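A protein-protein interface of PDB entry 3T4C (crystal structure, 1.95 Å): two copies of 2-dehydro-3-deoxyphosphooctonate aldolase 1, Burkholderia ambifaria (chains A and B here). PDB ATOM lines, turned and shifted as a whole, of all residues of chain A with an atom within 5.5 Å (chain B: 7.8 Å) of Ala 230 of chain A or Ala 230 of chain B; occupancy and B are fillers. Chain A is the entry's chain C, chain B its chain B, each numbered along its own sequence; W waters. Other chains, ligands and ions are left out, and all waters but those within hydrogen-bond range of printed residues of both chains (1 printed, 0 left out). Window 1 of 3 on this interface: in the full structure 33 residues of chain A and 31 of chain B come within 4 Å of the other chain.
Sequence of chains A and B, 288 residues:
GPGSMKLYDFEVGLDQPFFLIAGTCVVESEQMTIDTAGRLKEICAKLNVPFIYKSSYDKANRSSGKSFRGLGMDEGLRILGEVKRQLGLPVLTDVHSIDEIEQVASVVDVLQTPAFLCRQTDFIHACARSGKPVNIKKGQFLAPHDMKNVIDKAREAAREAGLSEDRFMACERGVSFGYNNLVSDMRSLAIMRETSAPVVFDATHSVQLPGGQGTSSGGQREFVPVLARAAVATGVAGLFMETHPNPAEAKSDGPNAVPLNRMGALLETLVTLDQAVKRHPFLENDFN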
ATOM      1  N   MET A 186      -3.683  -6.175 -26.593  1.00  0.00           N
ATOM      2  CA  MET A 186      -2.767  -5.716 -25.538  1.00  0.00           C
ATOM      3  C   MET A 186      -2.174  -6.886 -24.787  1.00  0.00           C
ATOM      4  O   MET A 186      -1.128  -6.730 -24.212  1.00  0.00           O
ATOM      5  CB  MET A 186      -3.457  -4.727 -24.585  1.00  0.00           C
ATOM      6  CG  MET A 186      -3.915  -3.452 -25.263  1.00  0.00           C
ATOM      7  SD  MET A 186      -2.541  -2.448 -25.833  1.00  0.00           S
ATOM      8  CE  MET A 186      -3.263  -1.630 -27.286  1.00  0.00           C
ATOM      9  N   LEU A 189       1.544  -7.728 -25.655  1.00  0.00           N
ATOM     10  CA  LEU A 189       2.602  -6.936 -25.066  1.00  0.00           C
ATOM     11  C   LEU A 189       3.117  -7.578 -23.778  1.00  0.00           C
ATOM     12  O   LEU A 189       4.304  -7.482 -23.464  1.00  0.00           O
ATOM     13  CB  LEU A 189       2.145  -5.512 -24.819  1.00  0.00           C
ATOM     14  CG  LEU A 189       1.692  -4.744 -26.053  1.00  0.00           C
ATOM     15  CD1 LEU A 189       1.071  -3.439 -25.583  1.00  0.00           C
ATOM     16  CD2 LEU A 189       2.840  -4.503 -27.070  1.00  0.00           C
ATOM     17  N   PRO A 225      -3.352   8.054 -30.426  1.00  0.00           N
ATOM     18  CA  PRO A 225      -3.322   8.382 -28.979  1.00  0.00           C
ATOM     19  C   PRO A 225      -3.965   7.322 -28.108  1.00  0.00           C
ATOM     20  O   PRO A 225      -3.416   6.971 -27.070  1.00  0.00           O
ATOM     21  CB  PRO A 225      -4.160   9.635 -28.886  1.00  0.00           C
ATOM     22  CG  PRO A 225      -4.132  10.237 -30.234  1.00  0.00           C
ATOM     23  CD  PRO A 225      -3.934   9.148 -31.222  1.00  0.00           C
ATOM     24  N   VAL A 226      -5.096   6.803 -28.575  1.00  0.00           N
ATOM     25  CA  VAL A 226      -5.833   5.712 -27.895  1.00  0.00           C
ATOM     26  C   VAL A 226      -4.927   4.520 -27.694  1.00  0.00           C
ATOM     27  O   VAL A 226      -4.734   4.007 -26.545  1.00  0.00           O
ATOM     28  CB  VAL A 226      -7.104   5.301 -28.678  1.00  0.00           C
ATOM     29  CG1 VAL A 226      -7.764   4.030 -28.100  1.00  0.00           C
ATOM     30  CG2 VAL A 226      -8.136   6.439 -28.702  1.00  0.00           C
ATOM     31  N   LEU A 227      -4.345   4.038 -28.792  1.00  0.00           N
ATOM     32  CA  LEU A 227      -3.544   2.867 -28.667  1.00  0.00           C
ATOM     33  C   LEU A 227      -2.235   3.133 -27.923  1.00  0.00           C
ATOM     34  O   LEU A 227      -1.746   2.246 -27.229  1.00  0.00           O
ATOM     35  CB  LEU A 227      -3.294   2.197 -30.009  1.00  0.00           C
ATOM     36  CG  LEU A 227      -4.534   1.660 -30.728  1.00  0.00           C
ATOM     37  CD1 LEU A 227      -4.038   0.842 -31.915  1.00  0.00           C
ATOM     38  CD2 LEU A 227      -5.427   0.798 -29.821  1.00  0.00           C
ATOM     39  N   ALA A 228      -1.645   4.310 -28.112  1.00  0.00           N
ATOM     40  CA  ALA A 228      -0.451   4.638 -27.399  1.00  0.00           C
ATOM     41  C   ALA A 228      -0.672   4.659 -25.899  1.00  0.00           C
ATOM     42  O   ALA A 228       0.162   4.150 -25.120  1.00  0.00           O
ATOM     43  CB  ALA A 228       0.144   5.997 -27.895  1.00  0.00           C
ATOM     44  N   ARG A 229      -1.756   5.268 -25.465  1.00  0.00           N
ATOM     45  CA  ARG A 229      -2.060   5.310 -24.001  1.00  0.00           C
ATOM     46  C   ARG A 229      -2.297   3.871 -23.462  1.00  0.00           C
ATOM     47  O   ARG A 229      -1.790   3.503 -22.431  1.00  0.00           O
ATOM     48  CB  ARG A 229      -3.278   6.190 -23.715  1.00  0.00           C
ATOM     49  CG  ARG A 229      -3.085   7.679 -23.848  1.00  0.00           C
ATOM     50  CD  ARG A 229      -4.170   8.478 -23.125  1.00  0.00           C
ATOM     51  NE  ARG A 229      -5.491   8.047 -23.530  1.00  0.00           N
ATOM     52  CZ  ARG A 229      -6.156   8.481 -24.595  1.00  0.00           C
ATOM     53  NH1 ARG A 229      -5.700   9.452 -25.352  1.00  0.00           N
ATOM     54  NH2 ARG A 229      -7.296   7.927 -24.914  1.00  0.00           N
ATOM     55  N   ALA A 230      -3.019   3.041 -24.211  1.00  0.00           N
ATOM     56  CA  ALA A 230      -3.345   1.696 -23.778  1.00  0.00           C
ATOM     57  C   ALA A 230      -2.077   0.838 -23.658  1.00  0.00           C
ATOM     58  O   ALA A 230      -1.937   0.044 -22.692  1.00  0.00           O
ATOM     59  CB  ALA A 230      -4.353   1.038 -24.743  1.00  0.00           C
ATOM     60  N   ALA A 231      -1.181   0.967 -24.656  1.00  0.00           N
ATOM     61  CA  ALA A 231       0.051   0.193 -24.721  1.00  0.00           C
ATOM     62  C   ALA A 231       1.009   0.589 -23.644  1.00  0.00           C
ATOM     63  O   ALA A 231       1.630  -0.275 -23.027  1.00  0.00           O
ATOM     64  CB  ALA A 231       0.717   0.313 -26.074  1.00  0.00           C
ATOM     65  N   VAL A 232       1.201   1.883 -23.448  1.00  0.00           N
ATOM     66  CA  VAL A 232       2.066   2.337 -22.375  1.00  0.00           C
ATOM     67  C   VAL A 232       1.563   1.929 -20.996  1.00  0.00           C
ATOM     68  O   VAL A 232       2.356   1.503 -20.165  1.00  0.00           O
ATOM     69  CB  VAL A 232       2.417   3.840 -22.511  1.00  0.00           C
ATOM     70  CG1 VAL A 232       3.221   4.380 -21.305  1.00  0.00           C
ATOM     71  CG2 VAL A 232       3.236   4.013 -23.762  1.00  0.00           C
ATOM     72  N   ALA A 233       0.260   2.032 -20.722  1.00  0.00           N
ATOM     73  CA  ALA A 233      -0.315   1.473 -19.473  1.00  0.00           C
ATOM     74  C   ALA A 233      -0.176  -0.050 -19.327  1.00  0.00           C
ATOM     75  O   ALA A 233      -0.064  -0.575 -18.174  1.00  0.00           O
ATOM     76  CB  ALA A 233      -1.814   1.909 -19.325  1.00  0.00           C
ATOM     77  N   THR A 234      -0.236  -0.770 -20.464  1.00  0.00           N
ATOM     78  CA  THR A 234      -0.009  -2.227 -20.481  1.00  0.00           C
ATOM     79  C   THR A 234       1.388  -2.517 -19.982  1.00  0.00           C
ATOM     80  O   THR A 234       1.595  -3.398 -19.168  1.00  0.00           O
ATOM     81  CB  THR A 234      -0.221  -2.823 -21.881  1.00  0.00           C
ATOM     82  OG1 THR A 234      -1.600  -2.621 -22.238  1.00  0.00           O
ATOM     83  CG2 THR A 234       0.093  -4.328 -21.888  1.00  0.00           C
ATOM     84  N   GLY A 235       2.339  -1.693 -20.400  1.00  0.00           N
ATOM     85  CA  GLY A 235       3.724  -1.828 -19.996  1.00  0.00           C
ATOM     86  C   GLY A 235       4.600  -2.280 -21.129  1.00  0.00           C
ATOM     87  O   GLY A 235       4.569  -3.444 -21.499  1.00  0.00           O
ATOM     88  N   SER B 184      -9.815  -7.679 -27.180  1.00  0.00           N
ATOM     89  CA  SER B 184     -10.282  -6.419 -26.642  1.00  0.00           C
ATOM     90  C   SER B 184      -9.757  -5.261 -27.490  1.00  0.00           C
ATOM     91  O   SER B 184      -8.597  -4.862 -27.364  1.00  0.00           O
ATOM     92  CB  SER B 184      -9.819  -6.288 -25.187  1.00  0.00           C
ATOM     93  OG  SER B 184     -10.649  -7.038 -24.325  1.00  0.00           O
ATOM     94  N   MET B 186      -9.257  -1.763 -28.115  1.00  0.00           N
ATOM     95  CA  MET B 186      -9.333  -0.506 -27.354  1.00  0.00           C
ATOM     96  C   MET B 186      -9.982   0.626 -28.164  1.00  0.00           C
ATOM     97  O   MET B 186     -10.556   1.515 -27.601  1.00  0.00           O
ATOM     98  CB  MET B 186      -7.927  -0.113 -26.855  1.00  0.00           C
ATOM     99  CG  MET B 186      -7.279  -1.135 -25.875  1.00  0.00           C
ATOM    100  SD  MET B 186      -8.274  -1.327 -24.361  1.00  0.00           S
ATOM    101  CE  MET B 186      -8.028  -3.084 -24.035  1.00  0.00           C
ATOM    102  N   ARG B 187      -9.963   0.559 -29.501  1.00  0.00           N
ATOM    103  CA  ARG B 187     -10.685   1.529 -30.331  1.00  0.00           C
ATOM    104  C   ARG B 187     -12.191   1.570 -29.969  1.00  0.00           C
ATOM    105  O   ARG B 187     -12.842   2.617 -30.082  1.00  0.00           O
ATOM    106  CB  ARG B 187     -10.518   1.196 -31.828  1.00  0.00           C
ATOM    107  CG  ARG B 187      -9.068   1.264 -32.321  1.00  0.00           C
ATOM    108  CD  ARG B 187      -8.913   0.857 -33.762  1.00  0.00           C
ATOM    109  NE  ARG B 187      -9.341  -0.507 -33.983  1.00  0.00           N
ATOM    110  CZ  ARG B 187      -9.185  -1.183 -35.116  1.00  0.00           C
ATOM    111  NH1 ARG B 187      -8.645  -0.605 -36.188  1.00  0.00           N
ATOM    112  NH2 ARG B 187      -9.586  -2.446 -35.176  1.00  0.00           N
ATOM    113  N   LEU B 189     -13.638   1.353 -27.158  1.00  0.00           N
ATOM    114  CA  LEU B 189     -13.917   2.186 -25.971  1.00  0.00           C
ATOM    115  C   LEU B 189     -14.065   3.653 -26.369  1.00  0.00           C
ATOM    116  O   LEU B 189     -14.812   4.425 -25.734  1.00  0.00           O
ATOM    117  CB  LEU B 189     -12.831   2.025 -24.923  1.00  0.00           C
ATOM    118  CG  LEU B 189     -12.669   0.612 -24.401  1.00  0.00           C
ATOM    119  CD1 LEU B 189     -11.427   0.543 -23.485  1.00  0.00           C
ATOM    120  CD2 LEU B 189     -13.959   0.090 -23.758  1.00  0.00           C
ATOM    121  N   PHE B 201     -15.953  -1.101 -19.099  1.00  0.00           N
ATOM    122  CA  PHE B 201     -15.082  -2.161 -19.612  1.00  0.00           C
ATOM    123  C   PHE B 201     -15.148  -3.411 -18.695  1.00  0.00           C
ATOM    124  O   PHE B 201     -14.838  -3.324 -17.505  1.00  0.00           O
ATOM    125  CB  PHE B 201     -13.625  -1.705 -19.666  1.00  0.00           C
ATOM    126  CG  PHE B 201     -12.708  -2.753 -20.239  1.00  0.00           C
ATOM    127  CD1 PHE B 201     -12.795  -3.060 -21.588  1.00  0.00           C
ATOM    128  CD2 PHE B 201     -11.816  -3.461 -19.442  1.00  0.00           C
ATOM    129  CE1 PHE B 201     -11.997  -4.021 -22.155  1.00  0.00           C
ATOM    130  CE2 PHE B 201     -11.004  -4.426 -19.994  1.00  0.00           C
ATOM    131  CZ  PHE B 201     -11.088  -4.711 -21.366  1.00  0.00           C
ATOM    132  N   PHE B 223      -4.242 -11.849 -17.643  1.00  0.00           N
ATOM    133  CA  PHE B 223      -4.625 -10.731 -18.551  1.00  0.00           C
ATOM    134  C   PHE B 223      -5.643  -9.736 -17.970  1.00  0.00           C
ATOM    135  O   PHE B 223      -5.870  -8.624 -18.522  1.00  0.00           O
ATOM    136  CB  PHE B 223      -5.031 -11.308 -19.919  1.00  0.00           C
ATOM    137  CG  PHE B 223      -3.929 -12.133 -20.549  1.00  0.00           C
ATOM    138  CD1 PHE B 223      -2.668 -11.560 -20.774  1.00  0.00           C
ATOM    139  CD2 PHE B 223      -4.087 -13.499 -20.792  1.00  0.00           C
ATOM    140  CE1 PHE B 223      -1.640 -12.285 -21.340  1.00  0.00           C
ATOM    141  CE2 PHE B 223      -3.062 -14.244 -21.363  1.00  0.00           C
ATOM    142  CZ  PHE B 223      -1.827 -13.643 -21.628  1.00  0.00           C
ATOM    143  N   VAL B 224      -6.205 -10.060 -16.806  1.00  0.00           N
ATOM    144  CA  VAL B 224      -7.156  -9.128 -16.173  1.00  0.00           C
ATOM    145  C   VAL B 224      -6.520  -7.785 -15.819  1.00  0.00           C
ATOM    146  O   VAL B 224      -7.035  -6.768 -16.253  1.00  0.00           O
ATOM    147  CB  VAL B 224      -7.909  -9.746 -14.996  1.00  0.00           C
ATOM    148  CG1 VAL B 224      -8.805  -8.716 -14.286  1.00  0.00           C
ATOM    149  CG2 VAL B 224      -8.765 -10.928 -15.510  1.00  0.00           C
ATOM    150  N   PRO B 225      -5.396  -7.769 -15.085  1.00  0.00           N
ATOM    151  CA  PRO B 225      -4.738  -6.486 -14.819  1.00  0.00           C
ATOM    152  C   PRO B 225      -4.226  -5.806 -16.102  1.00  0.00           C
ATOM    153  O   PRO B 225      -4.291  -4.596 -16.200  1.00  0.00           O
ATOM    154  CB  PRO B 225      -3.558  -6.838 -13.909  1.00  0.00           C
ATOM    155  CG  PRO B 225      -3.610  -8.329 -13.678  1.00  0.00           C
ATOM    156  CD  PRO B 225      -4.766  -8.914 -14.392  1.00  0.00           C
ATOM    157  N   VAL B 226      -3.723  -6.590 -17.051  1.00  0.00           N
ATOM    158  CA  VAL B 226      -3.278  -6.063 -18.342  1.00  0.00           C
ATOM    159  C   VAL B 226      -4.388  -5.267 -19.036  1.00  0.00           C
ATOM    160  O   VAL B 226      -4.196  -4.116 -19.406  1.00  0.00           O
ATOM    161  CB  VAL B 226      -2.753  -7.201 -19.284  1.00  0.00           C
ATOM    162  CG1 VAL B 226      -2.541  -6.706 -20.718  1.00  0.00           C
ATOM    163  CG2 VAL B 226      -1.465  -7.801 -18.716  1.00  0.00           C
ATOM    164  N   LEU B 227      -5.543  -5.901 -19.238  1.00  0.00           N
ATOM    165  CA  LEU B 227      -6.648  -5.270 -19.925  1.00  0.00           C
ATOM    166  C   LEU B 227      -7.302  -4.123 -19.124  1.00  0.00           C
ATOM    167  O   LEU B 227      -7.739  -3.118 -19.713  1.00  0.00           O
ATOM    168  CB  LEU B 227      -7.689  -6.300 -20.399  1.00  0.00           C
ATOM    169  CG  LEU B 227      -7.154  -7.334 -21.421  1.00  0.00           C
ATOM    170  CD1 LEU B 227      -8.337  -8.242 -21.808  1.00  0.00           C
ATOM    171  CD2 LEU B 227      -6.533  -6.708 -22.658  1.00  0.00           C
ATOM    172  N   ALA B 228      -7.304  -4.236 -17.807  1.00  0.00           N
ATOM    173  CA  ALA B 228      -7.851  -3.178 -16.956  1.00  0.00           C
ATOM    174  C   ALA B 228      -7.006  -1.921 -17.087  1.00  0.00           C
ATOM    175  O   ALA B 228      -7.581  -0.839 -17.259  1.00  0.00           O
ATOM    176  CB  ALA B 228      -7.939  -3.657 -15.510  1.00  0.00           C
ATOM    177  N   ARG B 229      -5.671  -2.067 -17.009  1.00  0.00           N
ATOM    178  CA  ARG B 229      -4.781  -0.910 -17.150  1.00  0.00           C
ATOM    179  C   ARG B 229      -4.953  -0.288 -18.559  1.00  0.00           C
ATOM    180  O   ARG B 229      -5.076   0.919 -18.708  1.00  0.00           O
ATOM    181  CB  ARG B 229      -3.311  -1.253 -16.895  1.00  0.00           C
ATOM    182  CG  ARG B 229      -2.888  -1.523 -15.467  1.00  0.00           C
ATOM    183  CD  ARG B 229      -1.365  -1.562 -15.313  1.00  0.00           C
ATOM    184  NE  ARG B 229      -0.727  -2.463 -16.290  1.00  0.00           N
ATOM    185  CZ  ARG B 229      -0.519  -3.764 -16.130  1.00  0.00           C
ATOM    186  NH1 ARG B 229       0.006  -4.472 -17.120  1.00  0.00           N
ATOM    187  NH2 ARG B 229      -0.842  -4.366 -14.997  1.00  0.00           N
ATOM    188  N   ALA B 230      -4.929  -1.130 -19.593  1.00  0.00           N
ATOM    189  CA  ALA B 230      -5.116  -0.643 -20.983  1.00  0.00           C
ATOM    190  C   ALA B 230      -6.420   0.109 -21.143  1.00  0.00           C
ATOM    191  O   ALA B 230      -6.426   1.177 -21.787  1.00  0.00           O
ATOM    192  CB  ALA B 230      -5.026  -1.790 -21.988  1.00  0.00           C
ATOM    193  N   ALA B 231      -7.529  -0.474 -20.649  1.00  0.00           N
ATOM    194  CA  ALA B 231      -8.868   0.097 -20.778  1.00  0.00           C
ATOM    195  C   ALA B 231      -8.965   1.404 -19.990  1.00  0.00           C
ATOM    196  O   ALA B 231      -9.464   2.413 -20.493  1.00  0.00           O
ATOM    197  CB  ALA B 231      -9.938  -0.907 -20.247  1.00  0.00           C
ATOM    198  N   VAL B 232      -8.474   1.404 -18.763  1.00  0.00           N
ATOM    199  CA  VAL B 232      -8.497   2.664 -17.947  1.00  0.00           C
ATOM    200  C   VAL B 232      -7.685   3.782 -18.587  1.00  0.00           C
ATOM    201  O   VAL B 232      -8.139   4.952 -18.631  1.00  0.00           O
ATOM    202  CB  VAL B 232      -8.145   2.414 -16.472  1.00  0.00           C
ATOM    203  CG1 VAL B 232      -8.079   3.736 -15.651  1.00  0.00           C
ATOM    204  CG2 VAL B 232      -9.236   1.523 -15.871  1.00  0.00           C
ATOM    205  N   ALA B 233      -6.535   3.447 -19.168  1.00  0.00           N
ATOM    206  CA  ALA B 233      -5.745   4.484 -19.877  1.00  0.00           C
ATOM    207  C   ALA B 233      -6.402   4.969 -21.159  1.00  0.00           C
ATOM    208  O   ALA B 233      -6.219   6.129 -21.566  1.00  0.00           O
ATOM    209  CB  ALA B 233      -4.298   4.004 -20.164  1.00  0.00           C
ATOM    210  N   THR B 234      -7.136   4.077 -21.845  1.00  0.00           N
ATOM    211  CA  THR B 234      -7.894   4.451 -23.024  1.00  0.00           C
ATOM    212  C   THR B 234      -8.923   5.515 -22.664  1.00  0.00           C
ATOM    213  O   THR B 234      -9.089   6.508 -23.403  1.00  0.00           O
ATOM    214  CB  THR B 234      -8.586   3.233 -23.645  1.00  0.00           C
ATOM    215  OG1 THR B 234      -7.571   2.336 -24.096  1.00  0.00           O
ATOM    216  CG2 THR B 234      -9.516   3.647 -24.838  1.00  0.00           C
ATOM    217  N   GLY B 235      -9.566   5.333 -21.514  1.00  0.00           N
ATOM    218  CA  GLY B 235     -10.532   6.286 -20.944  1.00  0.00           C
ATOM    219  C   GLY B 235     -11.928   5.693 -20.979  1.00  0.00           C
ATOM    220  O   GLY B 235     -12.511   5.513 -22.093  1.00  0.00           O
ATOM    221  N   VAL B 236     -12.407   5.286 -19.804  1.00  0.00           N
ATOM    222  CA  VAL B 236     -13.718   4.709 -19.620  1.00  0.00           C
ATOM    223  C   VAL B 236     -14.398   5.399 -18.452  1.00  0.00           C
ATOM    224  O   VAL B 236     -13.754   6.094 -17.668  1.00  0.00           O
ATOM    225  CB  VAL B 236     -13.635   3.157 -19.416  1.00  0.00           C
ATOM    226  CG1 VAL B 236     -13.063   2.453 -20.664  1.00  0.00           C
ATOM    227  CG2 VAL B 236     -12.818   2.773 -18.165  1.00  0.00           C
ATOM    228  N   LEU B 270      -4.848   1.715 -11.022  1.00  0.00           N
ATOM    229  CA  LEU B 270      -5.860   2.097 -11.946  1.00  0.00           C
ATOM    230  C   LEU B 270      -6.322   3.520 -11.661  1.00  0.00           C
ATOM    231  O   LEU B 270      -6.608   4.211 -12.599  1.00  0.00           O
ATOM    232  CB  LEU B 270      -7.041   1.115 -11.863  1.00  0.00           C
ATOM    233  CG  LEU B 270      -6.738  -0.316 -12.345  1.00  0.00           C
ATOM    234  CD1 LEU B 270      -7.930  -1.205 -12.022  1.00  0.00           C
ATOM    235  CD2 LEU B 270      -6.421  -0.378 -13.831  1.00  0.00           C
ATOM    236  N   LEU B 273      -3.801   5.894 -13.219  1.00  0.00           N
ATOM    237  CA  LEU B 273      -3.943   5.932 -14.691  1.00  0.00           C
ATOM    238  C   LEU B 273      -5.165   6.758 -15.110  1.00  0.00           C
ATOM    239  O   LEU B 273      -5.136   7.581 -16.067  1.00  0.00           O
ATOM    240  CB  LEU B 273      -4.090   4.499 -15.209  1.00  0.00           C
ATOM    241  CG  LEU B 273      -2.912   3.518 -15.021  1.00  0.00           C
ATOM    242  CD1 LEU B 273      -3.276   2.164 -15.638  1.00  0.00           C
ATOM    243  CD2 LEU B 273      -1.634   4.021 -15.644  1.00  0.00           C
ATOM    244  N   VAL B 277      -5.232  10.352 -17.345  1.00  0.00           N
ATOM    245  CA  VAL B 277      -5.789  10.539 -18.700  1.00  0.00           C
ATOM    246  C   VAL B 277      -6.946  11.503 -18.720  1.00  0.00           C
ATOM    247  O   VAL B 277      -7.383  11.955 -19.791  1.00  0.00           O
ATOM    248  CB  VAL B 277      -6.112   9.173 -19.356  1.00  0.00           C
ATOM    249  CG1 VAL B 277      -4.852   8.286 -19.280  1.00  0.00           C
ATOM    250  CG2 VAL B 277      -7.305   8.442 -18.743  1.00  0.00           C
HETATM  251  O   HOH W   1      -6.394  -5.847 -25.983  1.00  0.00           O
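NH1 of Arg 229 of chain B sits at hydrogen-bond distance from O of Thr 234 of chain A (2.8 Å).
The backbone carbonyl oxygen (O) of Thr 234 of chain B lies within hydrogen-bond range of the guanidinium group (NH2) of Arg 229 of chain A (2.7 Å).
The backbone carbonyl oxygen (O) of Ala 233 of chain A is in hydrogen-bond range of the guanidinium group (NE) of Arg 229 of chain B.
The guanidinium group (NE) of Arg 229 of chain A is in hydrogen-bond range of the backbone carbonyl oxygen (O) of Ala 233 of chain B (2.8 Å).
The side-chain hydroxyl (OG1) of Thr 234 of chain A lies close to the side-chain sulfur (SD) of Met 186 of chain A, 3.7 Å away.
The side-chain hydroxyl (OG1) of Thr 234 of chain A lies within hydrogen-bond range of the backbone carbonyl oxygen (O) of Ala 230 of chain A, at 2.7 Å.
SD of Met 186 of chain B sits close to OG1 of Thr 234 of chain B, 3.7 Å away.
The backbone carbonyl oxygen of Ala 230 of chain B sits at hydrogen-bond distance from the side-chain hydroxyl of Thr 234 of chain B (2.8 Å).
Among the printed residues, pairs that only touch across the chains: Met 186 of chain A with Val 226 of chain B, Met 186 of chain A with Ala 230 of chain B, Val 226 of chain A with Met 186 of chain B, Val 226 of chain A with Thr 234 of chain B, Leu 227 of chain A with Met 186 of chain B, Arg 229 of chain A with Val 277 of chain B, Ala 230 of chain A with Met 186 of chain B, Ala 230 of chain A with Ala 230 of chain B, Ala 230 of chain A with Thr 234 of chain B, Ala 233 of chain A with Ala 233 of chain B, Ala 233 of chain A with Leu 273 of chain B, Thr 234 of chain A with Val 226 of chain B and Thr 234 of chain A with Ala 230 of chain B.
Of the printed residues of chain B, Val 226 of chain A touches Met 186 (3.8 Å) and Thr 234 (3.7 Å).
Printed residues of chain B within 4 Å of Leu 227 of chain A: Met 186.
Of chain B, only Met 186, Ala 230 and Thr 234 come within 4 Å of Ala 230 of chain A.
No residue of chain B comes within 4 Å of Ala 231 of chain A.
Leu 189 of chain B touches none of the printed residues of chain A.
Leu 227 of chain B touches none of the printed residues of chain A.
Of the printed residues of chain A, Arg 229 of chain B touches Ala 233 and Thr 234.
Of the printed residues of chain A, Ala 230 of chain B touches Met 186, Ala 230 and Thr 234.
Printed residues of chain A within 4 Å of Thr 234 of chain B: Val 226, Arg 229 and Ala 230.
Of the printed residues of chain A, Leu 273 of chain B touches Ala 233.
Printed residues of chain B that touch a printed residue of chain A: Met 186, Val 226, Arg 229, Ala 230, Ala 233, Thr 234, Leu 273 and Val 277.
Hydrophobic or aromatic side chains of chain B that line the printed part of chain A: Met 186, Val 226, Ala 230, Ala 233, Leu 273 and Val 277.
Hydrophobic or aromatic side chains of chain A within 4 Å of the printed part of chain B: Met 186, Val 226, Leu 227, Ala 230 and Ala 233.
Among the printed residues, 17 pairs touch across the chains.
Among the printed residues, no Asp or Glu carboxylate lies within 4 Å of a Lys or Arg side-chain nitrogen of the other chain.
Arg 229 of chain A touches Ala 233 of chain B, and with the chains exchanged Ala 233 of chain A touches Arg 229 of chain B.
Arg 229 of chain A touches Thr 234 of chain B, and with the chains exchanged Thr 234 of chain A touches Arg 229 of chain B.
Ala 230 of chain A touches its own counterpart, Ala 230 of chain B.
Ala 233 of chain A touches its own counterpart, Ala 233 of chain B.
Water W1 lies within hydrogen-bond range of O of Ser 184 of chain B (2.8 Å) and N of Met 186 of chain A (2.8 Å).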
